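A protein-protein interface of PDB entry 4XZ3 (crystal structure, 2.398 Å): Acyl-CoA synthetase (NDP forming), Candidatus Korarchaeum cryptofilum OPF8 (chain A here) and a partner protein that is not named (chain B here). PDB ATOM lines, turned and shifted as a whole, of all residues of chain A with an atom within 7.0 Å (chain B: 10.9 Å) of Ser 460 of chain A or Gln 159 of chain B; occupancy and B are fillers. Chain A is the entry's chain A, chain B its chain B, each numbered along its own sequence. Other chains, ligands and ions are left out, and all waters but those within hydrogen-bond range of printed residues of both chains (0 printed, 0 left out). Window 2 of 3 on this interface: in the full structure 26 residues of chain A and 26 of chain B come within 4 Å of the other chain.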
ATOM      1  N   SER A 228     -27.688  -2.656  -9.469  1.00  0.00           N
ATOM      2  CA  SER A 228     -28.092  -4.047  -9.642  1.00  0.00           C
ATOM      3  C   SER A 228     -29.283  -4.346  -8.739  1.00  0.00           C
ATOM      4  O   SER A 228     -30.277  -4.939  -9.167  1.00  0.00           O
ATOM      5  CB  SER A 228     -26.927  -4.994  -9.341  1.00  0.00           C
ATOM      6  OG  SER A 228     -26.426  -4.782  -8.037  1.00  0.00           O
ATOM      7  N   GLN A 271     -23.598  -5.936 -15.974  1.00  0.00           N
ATOM      8  CA  GLN A 271     -23.552  -6.510 -14.633  1.00  0.00           C
ATOM      9  C   GLN A 271     -24.540  -5.852 -13.675  1.00  0.00           C
ATOM     10  O   GLN A 271     -24.886  -6.434 -12.649  1.00  0.00           O
ATOM     11  CB  GLN A 271     -22.142  -6.397 -14.062  1.00  0.00           C
ATOM     12  CG  GLN A 271     -21.107  -7.208 -14.818  1.00  0.00           C
ATOM     13  CD  GLN A 271     -19.697  -6.934 -14.335  1.00  0.00           C
ATOM     14  OE1 GLN A 271     -18.923  -6.251 -15.005  1.00  0.00           O
ATOM     15  NE2 GLN A 271     -19.359  -7.463 -13.165  1.00  0.00           N
ATOM     16  N   ARG A 454     -32.615  -8.555 -15.593  1.00  0.00           N
ATOM     17  CA  ARG A 454     -33.011  -8.921 -14.239  1.00  0.00           C
ATOM     18  C   ARG A 454     -32.560 -10.347 -13.931  1.00  0.00           C
ATOM     19  O   ARG A 454     -32.058 -10.631 -12.839  1.00  0.00           O
ATOM     20  CB  ARG A 454     -34.529  -8.778 -14.077  1.00  0.00           C
ATOM     21  CG  ARG A 454     -35.071  -9.227 -12.730  1.00  0.00           C
ATOM     22  CD  ARG A 454     -36.592  -9.150 -12.679  1.00  0.00           C
ATOM     23  NE  ARG A 454     -37.074  -7.787 -12.472  1.00  0.00           N
ATOM     24  CZ  ARG A 454     -38.356  -7.458 -12.322  1.00  0.00           C
ATOM     25  NH1 ARG A 454     -39.297  -8.396 -12.358  1.00  0.00           N
ATOM     26  NH2 ARG A 454     -38.701  -6.190 -12.131  1.00  0.00           N
ATOM     27  N   SER A 455     -32.735 -11.240 -14.899  1.00  0.00           N
ATOM     28  CA  SER A 455     -32.316 -12.630 -14.741  1.00  0.00           C
ATOM     29  C   SER A 455     -30.808 -12.742 -14.536  1.00  0.00           C
ATOM     30  O   SER A 455     -30.344 -13.579 -13.759  1.00  0.00           O
ATOM     31  CB  SER A 455     -32.734 -13.456 -15.952  1.00  0.00           C
ATOM     32  OG  SER A 455     -32.264 -14.789 -15.840  1.00  0.00           O
ATOM     33  N   TYR A 456     -30.048 -11.897 -15.228  1.00  0.00           N
ATOM     34  CA  TYR A 456     -28.595 -11.886 -15.084  1.00  0.00           C
ATOM     35  C   TYR A 456     -28.194 -11.598 -13.643  1.00  0.00           C
ATOM     36  O   TYR A 456     -27.392 -12.328 -13.054  1.00  0.00           O
ATOM     37  CB  TYR A 456     -27.957 -10.844 -16.009  1.00  0.00           C
ATOM     38  CG  TYR A 456     -26.444 -10.895 -16.020  1.00  0.00           C
ATOM     39  CD1 TYR A 456     -25.693 -10.253 -15.041  1.00  0.00           C
ATOM     40  CD2 TYR A 456     -25.766 -11.596 -17.007  1.00  0.00           C
ATOM     41  CE1 TYR A 456     -24.304 -10.309 -15.050  1.00  0.00           C
ATOM     42  CE2 TYR A 456     -24.389 -11.655 -17.027  1.00  0.00           C
ATOM     43  CZ  TYR A 456     -23.660 -11.012 -16.052  1.00  0.00           C
ATOM     44  OH  TYR A 456     -22.286 -11.095 -16.099  1.00  0.00           O
ATOM     45  N   VAL A 457     -28.759 -10.526 -13.092  1.00  0.00           N
ATOM     46  CA  VAL A 457     -28.455 -10.113 -11.731  1.00  0.00           C
ATOM     47  C   VAL A 457     -28.844 -11.214 -10.747  1.00  0.00           C
ATOM     48  O   VAL A 457     -28.088 -11.523  -9.819  1.00  0.00           O
ATOM     49  CB  VAL A 457     -29.184  -8.795 -11.369  1.00  0.00           C
ATOM     50  CG1 VAL A 457     -28.949  -8.419  -9.903  1.00  0.00           C
ATOM     51  CG2 VAL A 457     -28.722  -7.669 -12.283  1.00  0.00           C
ATOM     52  N   MET A 458     -30.025 -11.797 -10.952  1.00  0.00           N
ATOM     53  CA  MET A 458     -30.526 -12.852 -10.076  1.00  0.00           C
ATOM     54  C   MET A 458     -29.558 -14.029 -10.023  1.00  0.00           C
ATOM     55  O   MET A 458     -29.257 -14.543  -8.947  1.00  0.00           O
ATOM     56  CB  MET A 458     -31.904 -13.326 -10.540  1.00  0.00           C
ATOM     57  CG  MET A 458     -33.034 -12.370 -10.193  1.00  0.00           C
ATOM     58  SD  MET A 458     -33.451 -12.349  -8.288  1.00  0.00           S
ATOM     59  CE  MET A 458     -34.199 -14.143  -8.113  1.00  0.00           C
ATOM     60  N   LYS A 459     -29.062 -14.442 -11.184  1.00  0.00           N
ATOM     61  CA  LYS A 459     -28.127 -15.556 -11.250  1.00  0.00           C
ATOM     62  C   LYS A 459     -26.839 -15.236 -10.487  1.00  0.00           C
ATOM     63  O   LYS A 459     -26.363 -16.050  -9.700  1.00  0.00           O
ATOM     64  CB  LYS A 459     -27.821 -15.909 -12.707  1.00  0.00           C
ATOM     65  CG  LYS A 459     -28.970 -16.637 -13.403  1.00  0.00           C
ATOM     66  CD  LYS A 459     -28.707 -16.867 -14.887  1.00  0.00           C
ATOM     67  CE  LYS A 459     -28.846 -15.578 -15.691  1.00  0.00           C
ATOM     68  NZ  LYS A 459     -28.770 -15.801 -17.163  1.00  0.00           N
ATOM     69  N   SER A 460     -26.301 -14.038 -10.695  1.00  0.00           N
ATOM     70  CA  SER A 460     -25.062 -13.632 -10.034  1.00  0.00           C
ATOM     71  C   SER A 460     -25.219 -13.494  -8.517  1.00  0.00           C
ATOM     72  O   SER A 460     -24.243 -13.612  -7.783  1.00  0.00           O
ATOM     73  CB  SER A 460     -24.560 -12.312 -10.622  1.00  0.00           C
ATOM     74  OG  SER A 460     -25.616 -11.376 -10.736  1.00  0.00           O
ATOM     75  N   LEU A 461     -26.442 -13.244  -8.057  1.00  0.00           N
ATOM     76  CA  LEU A 461     -26.729 -13.156  -6.623  1.00  0.00           C
ATOM     77  C   LEU A 461     -27.256 -14.476  -6.070  1.00  0.00           C
ATOM     78  O   LEU A 461     -27.610 -14.569  -4.892  1.00  0.00           O
ATOM     79  CB  LEU A 461     -27.749 -12.055  -6.342  1.00  0.00           C
ATOM     80  CG  LEU A 461     -27.347 -10.625  -6.695  1.00  0.00           C
ATOM     81  CD1 LEU A 461     -28.526  -9.686  -6.460  1.00  0.00           C
ATOM     82  CD2 LEU A 461     -26.138 -10.182  -5.891  1.00  0.00           C
ATOM     83  N   ALA A 462     -27.327 -15.495  -6.922  1.00  0.00           N
ATOM     84  CA  ALA A 462     -27.862 -16.789  -6.517  1.00  0.00           C
ATOM     85  C   ALA A 462     -27.079 -17.360  -5.343  1.00  0.00           C
ATOM     86  O   ALA A 462     -25.864 -17.525  -5.416  1.00  0.00           O
ATOM     87  CB  ALA A 462     -27.841 -17.762  -7.684  1.00  0.00           C
ATOM     88  N   VAL A 463     -27.781 -17.665  -4.257  1.00  0.00           N
ATOM     89  CA  VAL A 463     -27.149 -18.247  -3.080  1.00  0.00           C
ATOM     90  C   VAL A 463     -26.561 -19.613  -3.429  1.00  0.00           C
ATOM     91  O   VAL A 463     -27.289 -20.599  -3.548  1.00  0.00           O
ATOM     92  CB  VAL A 463     -28.150 -18.379  -1.905  1.00  0.00           C
ATOM     93  CG1 VAL A 463     -27.530 -19.129  -0.724  1.00  0.00           C
ATOM     94  CG2 VAL A 463     -28.624 -17.003  -1.461  1.00  0.00           C
ATOM     95  N   ARG A 464     -25.243 -19.659  -3.599  1.00  0.00           N
ATOM     96  CA  ARG A 464     -24.554 -20.894  -3.953  1.00  0.00           C
ATOM     97  C   ARG A 464     -24.740 -21.949  -2.870  1.00  0.00           C
ATOM     98  O   ARG A 464     -24.537 -21.676  -1.687  1.00  0.00           O
ATOM     99  CB  ARG A 464     -23.061 -20.633  -4.175  1.00  0.00           C
ATOM    100  CG  ARG A 464     -22.750 -19.597  -5.245  1.00  0.00           C
ATOM    101  CD  ARG A 464     -21.266 -19.596  -5.580  1.00  0.00           C
ATOM    102  NE  ARG A 464     -20.435 -19.490  -4.380  1.00  0.00           N
ATOM    103  CZ  ARG A 464     -19.827 -18.383  -3.963  1.00  0.00           C
ATOM    104  NH1 ARG A 464     -19.932 -17.247  -4.643  1.00  0.00           N
ATOM    105  NH2 ARG A 464     -19.098 -18.412  -2.855  1.00  0.00           N
ATOM    106  OXT ARG A 464     -25.091 -23.095  -3.155  1.00  0.00           O
ATOM    107  N   PHE B 136     -11.144 -11.345 -20.939  1.00  0.00           N
ATOM    108  CA  PHE B 136     -10.995 -12.693 -21.478  1.00  0.00           C
ATOM    109  C   PHE B 136     -11.165 -12.677 -22.991  1.00  0.00           C
ATOM    110  O   PHE B 136     -11.826 -11.793 -23.535  1.00  0.00           O
ATOM    111  CB  PHE B 136     -12.010 -13.641 -20.842  1.00  0.00           C
ATOM    112  CG  PHE B 136     -12.037 -15.004 -21.463  1.00  0.00           C
ATOM    113  CD1 PHE B 136     -11.038 -15.923 -21.191  1.00  0.00           C
ATOM    114  CD2 PHE B 136     -13.060 -15.370 -22.316  1.00  0.00           C
ATOM    115  CE1 PHE B 136     -11.060 -17.180 -21.761  1.00  0.00           C
ATOM    116  CE2 PHE B 136     -13.088 -16.627 -22.887  1.00  0.00           C
ATOM    117  CZ  PHE B 136     -12.086 -17.532 -22.607  1.00  0.00           C
ATOM    118  N   SER B 150     -14.039  -9.927 -23.896  1.00  0.00           N
ATOM    119  CA  SER B 150     -15.118  -9.536 -23.000  1.00  0.00           C
ATOM    120  C   SER B 150     -14.529  -8.990 -21.698  1.00  0.00           C
ATOM    121  O   SER B 150     -13.403  -9.332 -21.335  1.00  0.00           O
ATOM    122  CB  SER B 150     -16.037 -10.720 -22.715  1.00  0.00           C
ATOM    123  OG  SER B 150     -15.312 -11.794 -22.146  1.00  0.00           O
ATOM    124  N   PHE B 151     -15.291  -8.145 -21.007  1.00  0.00           N
ATOM    125  CA  PHE B 151     -14.837  -7.523 -19.762  1.00  0.00           C
ATOM    126  C   PHE B 151     -15.832  -7.745 -18.628  1.00  0.00           C
ATOM    127  O   PHE B 151     -17.033  -7.856 -18.861  1.00  0.00           O
ATOM    128  CB  PHE B 151     -14.619  -6.022 -19.948  1.00  0.00           C
ATOM    129  CG  PHE B 151     -13.577  -5.675 -20.966  1.00  0.00           C
ATOM    130  CD1 PHE B 151     -13.913  -5.549 -22.304  1.00  0.00           C
ATOM    131  CD2 PHE B 151     -12.263  -5.460 -20.583  1.00  0.00           C
ATOM    132  CE1 PHE B 151     -12.952  -5.221 -23.246  1.00  0.00           C
ATOM    133  CE2 PHE B 151     -11.300  -5.132 -21.518  1.00  0.00           C
ATOM    134  CZ  PHE B 151     -11.647  -5.012 -22.853  1.00  0.00           C
ATOM    135  N   ARG B 152     -15.318  -7.818 -17.405  1.00  0.00           N
ATOM    136  CA  ARG B 152     -16.155  -7.900 -16.214  1.00  0.00           C
ATOM    137  C   ARG B 152     -15.448  -7.231 -15.037  1.00  0.00           C
ATOM    138  O   ARG B 152     -14.234  -7.371 -14.874  1.00  0.00           O
ATOM    139  CB  ARG B 152     -16.487  -9.355 -15.867  1.00  0.00           C
ATOM    140  CG  ARG B 152     -17.444 -10.054 -16.823  1.00  0.00           C
ATOM    141  CD  ARG B 152     -18.818  -9.398 -16.844  1.00  0.00           C
ATOM    142  NE  ARG B 152     -19.803 -10.231 -17.529  1.00  0.00           N
ATOM    143  CZ  ARG B 152     -19.979 -10.269 -18.847  1.00  0.00           C
ATOM    144  NH1 ARG B 152     -19.232  -9.523 -19.653  1.00  0.00           N
ATOM    145  NH2 ARG B 152     -20.903 -11.067 -19.366  1.00  0.00           N
ATOM    146  N   VAL B 153     -16.205  -6.488 -14.237  1.00  0.00           N
ATOM    147  CA  VAL B 153     -15.659  -5.835 -13.057  1.00  0.00           C
ATOM    148  C   VAL B 153     -15.566  -6.838 -11.904  1.00  0.00           C
ATOM    149  O   VAL B 153     -16.530  -7.539 -11.600  1.00  0.00           O
ATOM    150  CB  VAL B 153     -16.520  -4.627 -12.632  1.00  0.00           C
ATOM    151  CG1 VAL B 153     -15.922  -3.942 -11.405  1.00  0.00           C
ATOM    152  CG2 VAL B 153     -16.647  -3.642 -13.777  1.00  0.00           C
ATOM    153  N   PRO B 155     -14.966  -8.129  -7.871  1.00  0.00           N
ATOM    154  CA  PRO B 155     -14.823  -9.590  -7.940  1.00  0.00           C
ATOM    155  C   PRO B 155     -15.878 -10.233  -8.830  1.00  0.00           C
ATOM    156  O   PRO B 155     -16.998  -9.729  -8.933  1.00  0.00           O
ATOM    157  CB  PRO B 155     -14.991 -10.031  -6.485  1.00  0.00           C
ATOM    158  CG  PRO B 155     -15.794  -8.959  -5.854  1.00  0.00           C
ATOM    159  CD  PRO B 155     -15.388  -7.685  -6.531  1.00  0.00           C
ATOM    160  N   LEU B 156     -15.511 -11.344  -9.458  1.00  0.00           N
ATOM    161  CA  LEU B 156     -16.379 -12.031 -10.405  1.00  0.00           C
ATOM    162  C   LEU B 156     -17.180 -13.140  -9.757  1.00  0.00           C
ATOM    163  O   LEU B 156     -16.626 -13.979  -9.048  1.00  0.00           O
ATOM    164  CB  LEU B 156     -15.553 -12.620 -11.551  1.00  0.00           C
ATOM    165  CG  LEU B 156     -15.344 -11.736 -12.780  1.00  0.00           C
ATOM    166  CD1 LEU B 156     -14.851 -10.358 -12.390  1.00  0.00           C
ATOM    167  CD2 LEU B 156     -14.372 -12.405 -13.731  1.00  0.00           C
ATOM    168  N   SER B 157     -18.486 -13.134 -10.006  1.00  0.00           N
ATOM    169  CA  SER B 157     -19.342 -14.263  -9.663  1.00  0.00           C
ATOM    170  C   SER B 157     -19.157 -15.356 -10.702  1.00  0.00           C
ATOM    171  O   SER B 157     -18.567 -15.118 -11.760  1.00  0.00           O
ATOM    172  CB  SER B 157     -20.812 -13.839  -9.595  1.00  0.00           C
ATOM    173  OG  SER B 157     -21.239 -13.201 -10.792  1.00  0.00           O
ATOM    174  N   GLU B 158     -19.649 -16.553 -10.403  1.00  0.00           N
ATOM    175  CA  GLU B 158     -19.559 -17.650 -11.353  1.00  0.00           C
ATOM    176  C   GLU B 158     -20.366 -17.295 -12.597  1.00  0.00           C
ATOM    177  O   GLU B 158     -20.000 -17.661 -13.710  1.00  0.00           O
ATOM    178  CB  GLU B 158     -20.053 -18.957 -10.731  1.00  0.00           C
ATOM    179  CG  GLU B 158     -19.709 -20.187 -11.557  1.00  0.00           C
ATOM    180  CD  GLU B 158     -20.023 -21.485 -10.839  1.00  0.00           C
ATOM    181  OE1 GLU B 158     -20.576 -21.433  -9.720  1.00  0.00           O
ATOM    182  OE2 GLU B 158     -19.708 -22.559 -11.394  1.00  0.00           O
ATOM    183  N   GLN B 159     -21.442 -16.538 -12.403  1.00  0.00           N
ATOM    184  CA  GLN B 159     -22.252 -16.069 -13.518  1.00  0.00           C
ATOM    185  C   GLN B 159     -21.428 -15.159 -14.424  1.00  0.00           C
ATOM    186  O   GLN B 159     -21.372 -15.382 -15.637  1.00  0.00           O
ATOM    187  CB  GLN B 159     -23.495 -15.333 -13.007  1.00  0.00           C
ATOM    188  CG  GLN B 159     -24.334 -14.672 -14.095  1.00  0.00           C
ATOM    189  CD  GLN B 159     -24.903 -15.668 -15.092  1.00  0.00           C
ATOM    190  OE1 GLN B 159     -24.902 -16.876 -14.853  1.00  0.00           O
ATOM    191  NE2 GLN B 159     -25.392 -15.161 -16.218  1.00  0.00           N
ATOM    192  N   ASP B 160     -20.774 -14.165 -13.823  1.00  0.00           N
ATOM    193  CA  ASP B 160     -19.912 -13.244 -14.558  1.00  0.00           C
ATOM    194  C   ASP B 160     -18.873 -13.982 -15.391  1.00  0.00           C
ATOM    195  O   ASP B 160     -18.731 -13.730 -16.587  1.00  0.00           O
ATOM    196  CB  ASP B 160     -19.195 -12.288 -13.594  1.00  0.00           C
ATOM    197  CG  ASP B 160     -20.127 -11.263 -12.977  1.00  0.00           C
ATOM    198  OD1 ASP B 160     -21.098 -10.854 -13.651  1.00  0.00           O
ATOM    199  OD2 ASP B 160     -19.885 -10.868 -11.815  1.00  0.00           O
ATOM    200  N   ALA B 161     -18.147 -14.894 -14.753  1.00  0.00           N
ATOM    201  CA  ALA B 161     -17.081 -15.617 -15.433  1.00  0.00           C
ATOM    202  C   ALA B 161     -17.641 -16.511 -16.534  1.00  0.00           C
ATOM    203  O   ALA B 161     -17.067 -16.602 -17.618  1.00  0.00           O
ATOM    204  CB  ALA B 161     -16.283 -16.441 -14.437  1.00  0.00           C
ATOM    205  N   GLU B 162     -18.775 -17.145 -16.258  1.00  0.00           N
ATOM    206  CA  GLU B 162     -19.383 -18.073 -17.204  1.00  0.00           C
ATOM    207  C   GLU B 162     -19.950 -17.333 -18.420  1.00  0.00           C
ATOM    208  O   GLU B 162     -19.828 -17.795 -19.559  1.00  0.00           O
ATOM    209  CB  GLU B 162     -20.478 -18.878 -16.503  1.00  0.00           C
ATOM    210  CG  GLU B 162     -21.131 -19.953 -17.355  1.00  0.00           C
ATOM    211  CD  GLU B 162     -22.090 -20.824 -16.560  1.00  0.00           C
ATOM    212  OE1 GLU B 162     -23.083 -21.306 -17.147  1.00  0.00           O
ATOM    213  OE2 GLU B 162     -21.848 -21.034 -15.351  1.00  0.00           O
ATOM    214  N   SER B 163     -20.519 -16.152 -18.184  1.00  0.00           N
ATOM    215  CA  SER B 163     -21.184 -15.409 -19.250  1.00  0.00           C
ATOM    216  C   SER B 163     -20.166 -14.696 -20.138  1.00  0.00           C
ATOM    217  O   SER B 163     -20.370 -14.573 -21.350  1.00  0.00           O
ATOM    218  CB  SER B 163     -22.187 -14.398 -18.670  1.00  0.00           C
ATOM    219  OG  SER B 163     -21.566 -13.445 -17.815  1.00  0.00           O
ATOM    220  N   MET B 164     -19.063 -14.246 -19.547  1.00  0.00           N
ATOM    221  CA  MET B 164     -18.052 -13.531 -20.316  1.00  0.00           C
ATOM    222  C   MET B 164     -17.283 -14.491 -21.231  1.00  0.00           C
ATOM    223  O   MET B 164     -16.586 -14.061 -22.153  1.00  0.00           O
ATOM    224  CB  MET B 164     -17.095 -12.778 -19.387  1.00  0.00           C
ATOM    225  CG  MET B 164     -15.939 -13.591 -18.845  1.00  0.00           C
ATOM    226  SD  MET B 164     -14.913 -12.610 -17.493  1.00  0.00           S
ATOM    227  CE  MET B 164     -14.033 -11.295 -18.643  1.00  0.00           C
ATOM    228  N   ILE B 165     -17.421 -15.790 -20.978  1.00  0.00           N
ATOM    229  CA  ILE B 165     -16.822 -16.801 -21.838  1.00  0.00           C
ATOM    230  C   ILE B 165     -17.739 -17.122 -23.008  1.00  0.00           C
ATOM    231  O   ILE B 165     -17.286 -17.233 -24.143  1.00  0.00           O
ATOM    232  CB  ILE B 165     -16.516 -18.101 -21.060  1.00  0.00           C
ATOM    233  CG1 ILE B 165     -15.378 -17.854 -20.068  1.00  0.00           C
ATOM    234  CG2 ILE B 165     -16.135 -19.235 -22.018  1.00  0.00           C
ATOM    235  CD1 ILE B 165     -15.117 -19.008 -19.120  1.00  0.00           C
ATOM    236  N   LYS B 166     -19.030 -17.275 -22.733  1.00  0.00           N
ATOM    237  CA  LYS B 166     -19.970 -17.623 -23.789  1.00  0.00           C
ATOM    238  C   LYS B 166     -20.212 -16.483 -24.774  1.00  0.00           C
ATOM    239  O   LYS B 166     -20.683 -16.725 -25.885  1.00  0.00           O
ATOM    240  CB  LYS B 166     -21.306 -18.059 -23.189  1.00  0.00           C
ATOM    241  CG  LYS B 166     -21.277 -19.419 -22.518  1.00  0.00           C
ATOM    242  CD  LYS B 166     -22.661 -19.808 -22.025  1.00  0.00           C
ATOM    243  CE  LYS B 166     -22.718 -21.263 -21.586  1.00  0.00           C
ATOM    244  NZ  LYS B 166     -21.836 -21.538 -20.419  1.00  0.00           N
ATOM    245  N   GLU B 167     -19.888 -15.252 -24.385  1.00  0.00           N
ATOM    246  CA  GLU B 167     -20.205 -14.105 -25.235  1.00  0.00           C
ATOM    247  C   GLU B 167     -19.183 -13.888 -26.361  1.00  0.00           C
ATOM    248  O   GLU B 167     -19.539 -13.358 -27.414  1.00  0.00           O
ATOM    249  CB  GLU B 167     -20.362 -12.826 -24.400  1.00  0.00           C
ATOM    250  CG  GLU B 167     -19.109 -12.273 -23.756  1.00  0.00           C
ATOM    251  CD  GLU B 167     -19.349 -10.894 -23.149  1.00  0.00           C
ATOM    252  OE1 GLU B 167     -19.738  -9.972 -23.900  1.00  0.00           O
ATOM    253  OE2 GLU B 167     -19.169 -10.730 -21.923  1.00  0.00           O
ATOM    254  N   ILE B 185     -13.513 -25.905 -19.588  1.00  0.00           N
ATOM    255  CA  ILE B 185     -14.077 -24.575 -19.364  1.00  0.00           C
ATOM    256  C   ILE B 185     -14.062 -24.202 -17.881  1.00  0.00           C
ATOM    257  O   ILE B 185     -13.913 -23.032 -17.534  1.00  0.00           O
ATOM    258  CB  ILE B 185     -15.520 -24.480 -19.912  1.00  0.00           C
ATOM    259  CG1 ILE B 185     -15.499 -24.585 -21.443  1.00  0.00           C
ATOM    260  CG2 ILE B 185     -16.181 -23.170 -19.486  1.00  0.00           C
ATOM    261  CD1 ILE B 185     -16.872 -24.605 -22.096  1.00  0.00           C
ATOM    262  N   GLU B 186     -14.235 -25.191 -17.013  1.00  0.00           N
ATOM    263  CA  GLU B 186     -14.269 -24.937 -15.580  1.00  0.00           C
ATOM    264  C   GLU B 186     -12.931 -24.394 -15.093  1.00  0.00           C
ATOM    265  O   GLU B 186     -12.883 -23.493 -14.248  1.00  0.00           O
ATOM    266  CB  GLU B 186     -14.636 -26.213 -14.822  1.00  0.00           C
ATOM    267  CG  GLU B 186     -16.032 -26.728 -15.139  1.00  0.00           C
ATOM    268  CD  GLU B 186     -17.117 -25.711 -14.822  1.00  0.00           C
ATOM    269  OE1 GLU B 186     -18.174 -25.730 -15.491  1.00  0.00           O
ATOM    270  OE2 GLU B 186     -16.912 -24.893 -13.901  1.00  0.00           O
ATOM    271  N   LYS B 189     -12.846 -20.771 -16.006  1.00  0.00           N
ATOM    272  CA  LYS B 189     -13.681 -19.980 -15.110  1.00  0.00           C
ATOM    273  C   LYS B 189     -12.954 -19.714 -13.803  1.00  0.00           C
ATOM    274  O   LYS B 189     -12.959 -18.591 -13.294  1.00  0.00           O
ATOM    275  CB  LYS B 189     -15.008 -20.687 -14.837  1.00  0.00           C
ATOM    276  CG  LYS B 189     -15.940 -20.751 -16.033  1.00  0.00           C
ATOM    277  CD  LYS B 189     -17.115 -21.688 -15.779  1.00  0.00           C
ATOM    278  CE  LYS B 189     -17.918 -21.271 -14.550  1.00  0.00           C
ATOM    279  NZ  LYS B 189     -19.143 -22.098 -14.370  1.00  0.00           N
ATOM    280  N   ASP B 190     -12.338 -20.759 -13.265  1.00  0.00           N
ATOM    281  CA  ASP B 190     -11.611 -20.655 -12.013  1.00  0.00           C
ATOM    282  C   ASP B 190     -10.467 -19.660 -12.162  1.00  0.00           C
ATOM    283  O   ASP B 190     -10.234 -18.829 -11.284  1.00  0.00           O
ATOM    284  CB  ASP B 190     -11.081 -22.028 -11.594  1.00  0.00           C
ATOM    285  CG  ASP B 190     -10.636 -22.068 -10.144  1.00  0.00           C
ATOM    286  OD1 ASP B 190     -11.393 -21.593  -9.270  1.00  0.00           O
ATOM    287  OD2 ASP B 190      -9.526 -22.579  -9.879  1.00  0.00           O
ATOM    288  N   LEU B 192     -10.289 -17.172 -14.218  1.00  0.00           N
ATOM    289  CA  LEU B 192     -10.846 -15.828 -14.331  1.00  0.00           C
ATOM    290  C   LEU B 192     -11.208 -15.268 -12.963  1.00  0.00           C
ATOM    291  O   LEU B 192     -10.878 -14.122 -12.641  1.00  0.00           O
ATOM    292  CB  LEU B 192     -12.079 -15.833 -15.237  1.00  0.00           C
ATOM    293  CG  LEU B 192     -11.792 -16.020 -16.729  1.00  0.00           C
ATOM    294  CD1 LEU B 192     -13.069 -16.342 -17.489  1.00  0.00           C
ATOM    295  CD2 LEU B 192     -11.120 -14.781 -17.308  1.00  0.00           C
ATOM    296  N   ILE B 193     -11.875 -16.086 -12.155  1.00  0.00           N
ATOM    297  CA  ILE B 193     -12.274 -15.671 -10.816  1.00  0.00           C
ATOM    298  C   ILE B 193     -11.045 -15.340  -9.981  1.00  0.00           C
ATOM    299  O   ILE B 193     -11.011 -14.329  -9.279  1.00  0.00           O
ATOM    300  CB  ILE B 193     -13.108 -16.762 -10.114  1.00  0.00           C
ATOM    301  CG1 ILE B 193     -14.414 -16.992 -10.879  1.00  0.00           C
ATOM    302  CG2 ILE B 193     -13.418 -16.366  -8.670  1.00  0.00           C
ATOM    303  CD1 ILE B 193     -15.148 -18.257 -10.483  1.00  0.00           C
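The backbone NH (N) of Val 153 of chain B lies within hydrogen-bond range of the side-chain amide oxygen (OE1) of Gln 271 of chain A (2.8 Å). OH of Tyr 456 of chain A is in hydrogen-bond range of NE of Arg 152 of chain B, at 3.0 Å. The side-chain hydroxyl of Tyr 456 of chain A sits at hydrogen-bond distance from the side-chain carboxylate of Asp 160 of chain B, at 2.7 Å. The side-chain hydroxyl (OG) of Ser 163 of chain B sits at hydrogen-bond distance from the side-chain hydroxyl (OH) of Tyr 456 of chain A (3.0 Å).
Of chain A, only Tyr 456, Lys 459 and Ser 460 come within 4 Å of Gln 159 of chain B. Of chain B, only Arg 152, Gln 159, Asp 160 and Ser 163 come within 4 Å of Tyr 456 of chain A. No residue of chain B comes within 4 Å of Val 457 of chain A. Of chain B, only Gln 159 (3.5 Å) comes within 4 Å of Lys 459 of chain A. Printed residues of chain A within 4 Å of Val 153 of chain B: Gln 271 (2.8 Å). Printed residues of chain A within 4 Å of Ser 157 of chain B: Ser 460. Printed residues of chain B within 4 Å of Gln 271 of chain A: Arg 152, Val 153 and Asp 160. The nearest residue of chain A that does not touch Gln 159 of chain B is Ser 455 of chain A (5.8 Å).
Arg 152 of chain B touches Gln 271 of chain A. NE2 of Gln 271 of chain A touches OD2 of Asp 160 of chain B, at 3.7 Å. CD2 of Tyr 456 of chain A touches NE2 of Gln 159 of chain B, 3.7 Å away. Gln 159 of chain B touches Lys 459 of chain A. Ser 157 of chain B touches Ser 460 of chain A (OG to CB, 3.4 Å). CA of Ser 460 of chain A touches CB of Gln 159 of chain B (3.8 Å).
The side-chain hydroxyl of Ser 460 of chain A sits at hydrogen-bond distance from the backbone carbonyl oxygen of Tyr 456 of chain A (3.1 Å). OG of Ser 460 of chain A sits at hydrogen-bond distance from O of Val 457 of chain A. OE2 of Glu 167 of chain B lies within salt-bridge range of NH1 of Arg 152 of chain B (2.6 Å). The side-chain carboxylate (OD2) of Asp 160 of chain B lies within hydrogen-bond range of the side-chain hydroxyl (OG) of Ser 157 of chain B, at 2.9 Å. O of Gln 159 of chain B sits at hydrogen-bond distance from OG of Ser 163 of chain B, 2.9 Å away. The side-chain hydroxyl (OG) of Ser 163 of chain B lies within hydrogen-bond range of the backbone carbonyl oxygen (O) of Asp 160 of chain B (3.1 Å).
Of the 13 printed residues of chain A, 4 touch a printed residue of chain B. Hydrophobic or aromatic side chains of chain A that line the printed part of chain B: Tyr 456. Of the 24 printed residues of chain B, 6 touch a printed residue of chain A. Hydrophobic or aromatic side chains of chain B that line the printed part of chain A: Val 153. Among the printed residues, 10 pairs touch across the chains. Among the printed residues, no Asp or Glu carboxylate lies within 4 Å of a Lys or Arg side-chain nitrogen of the other chain.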
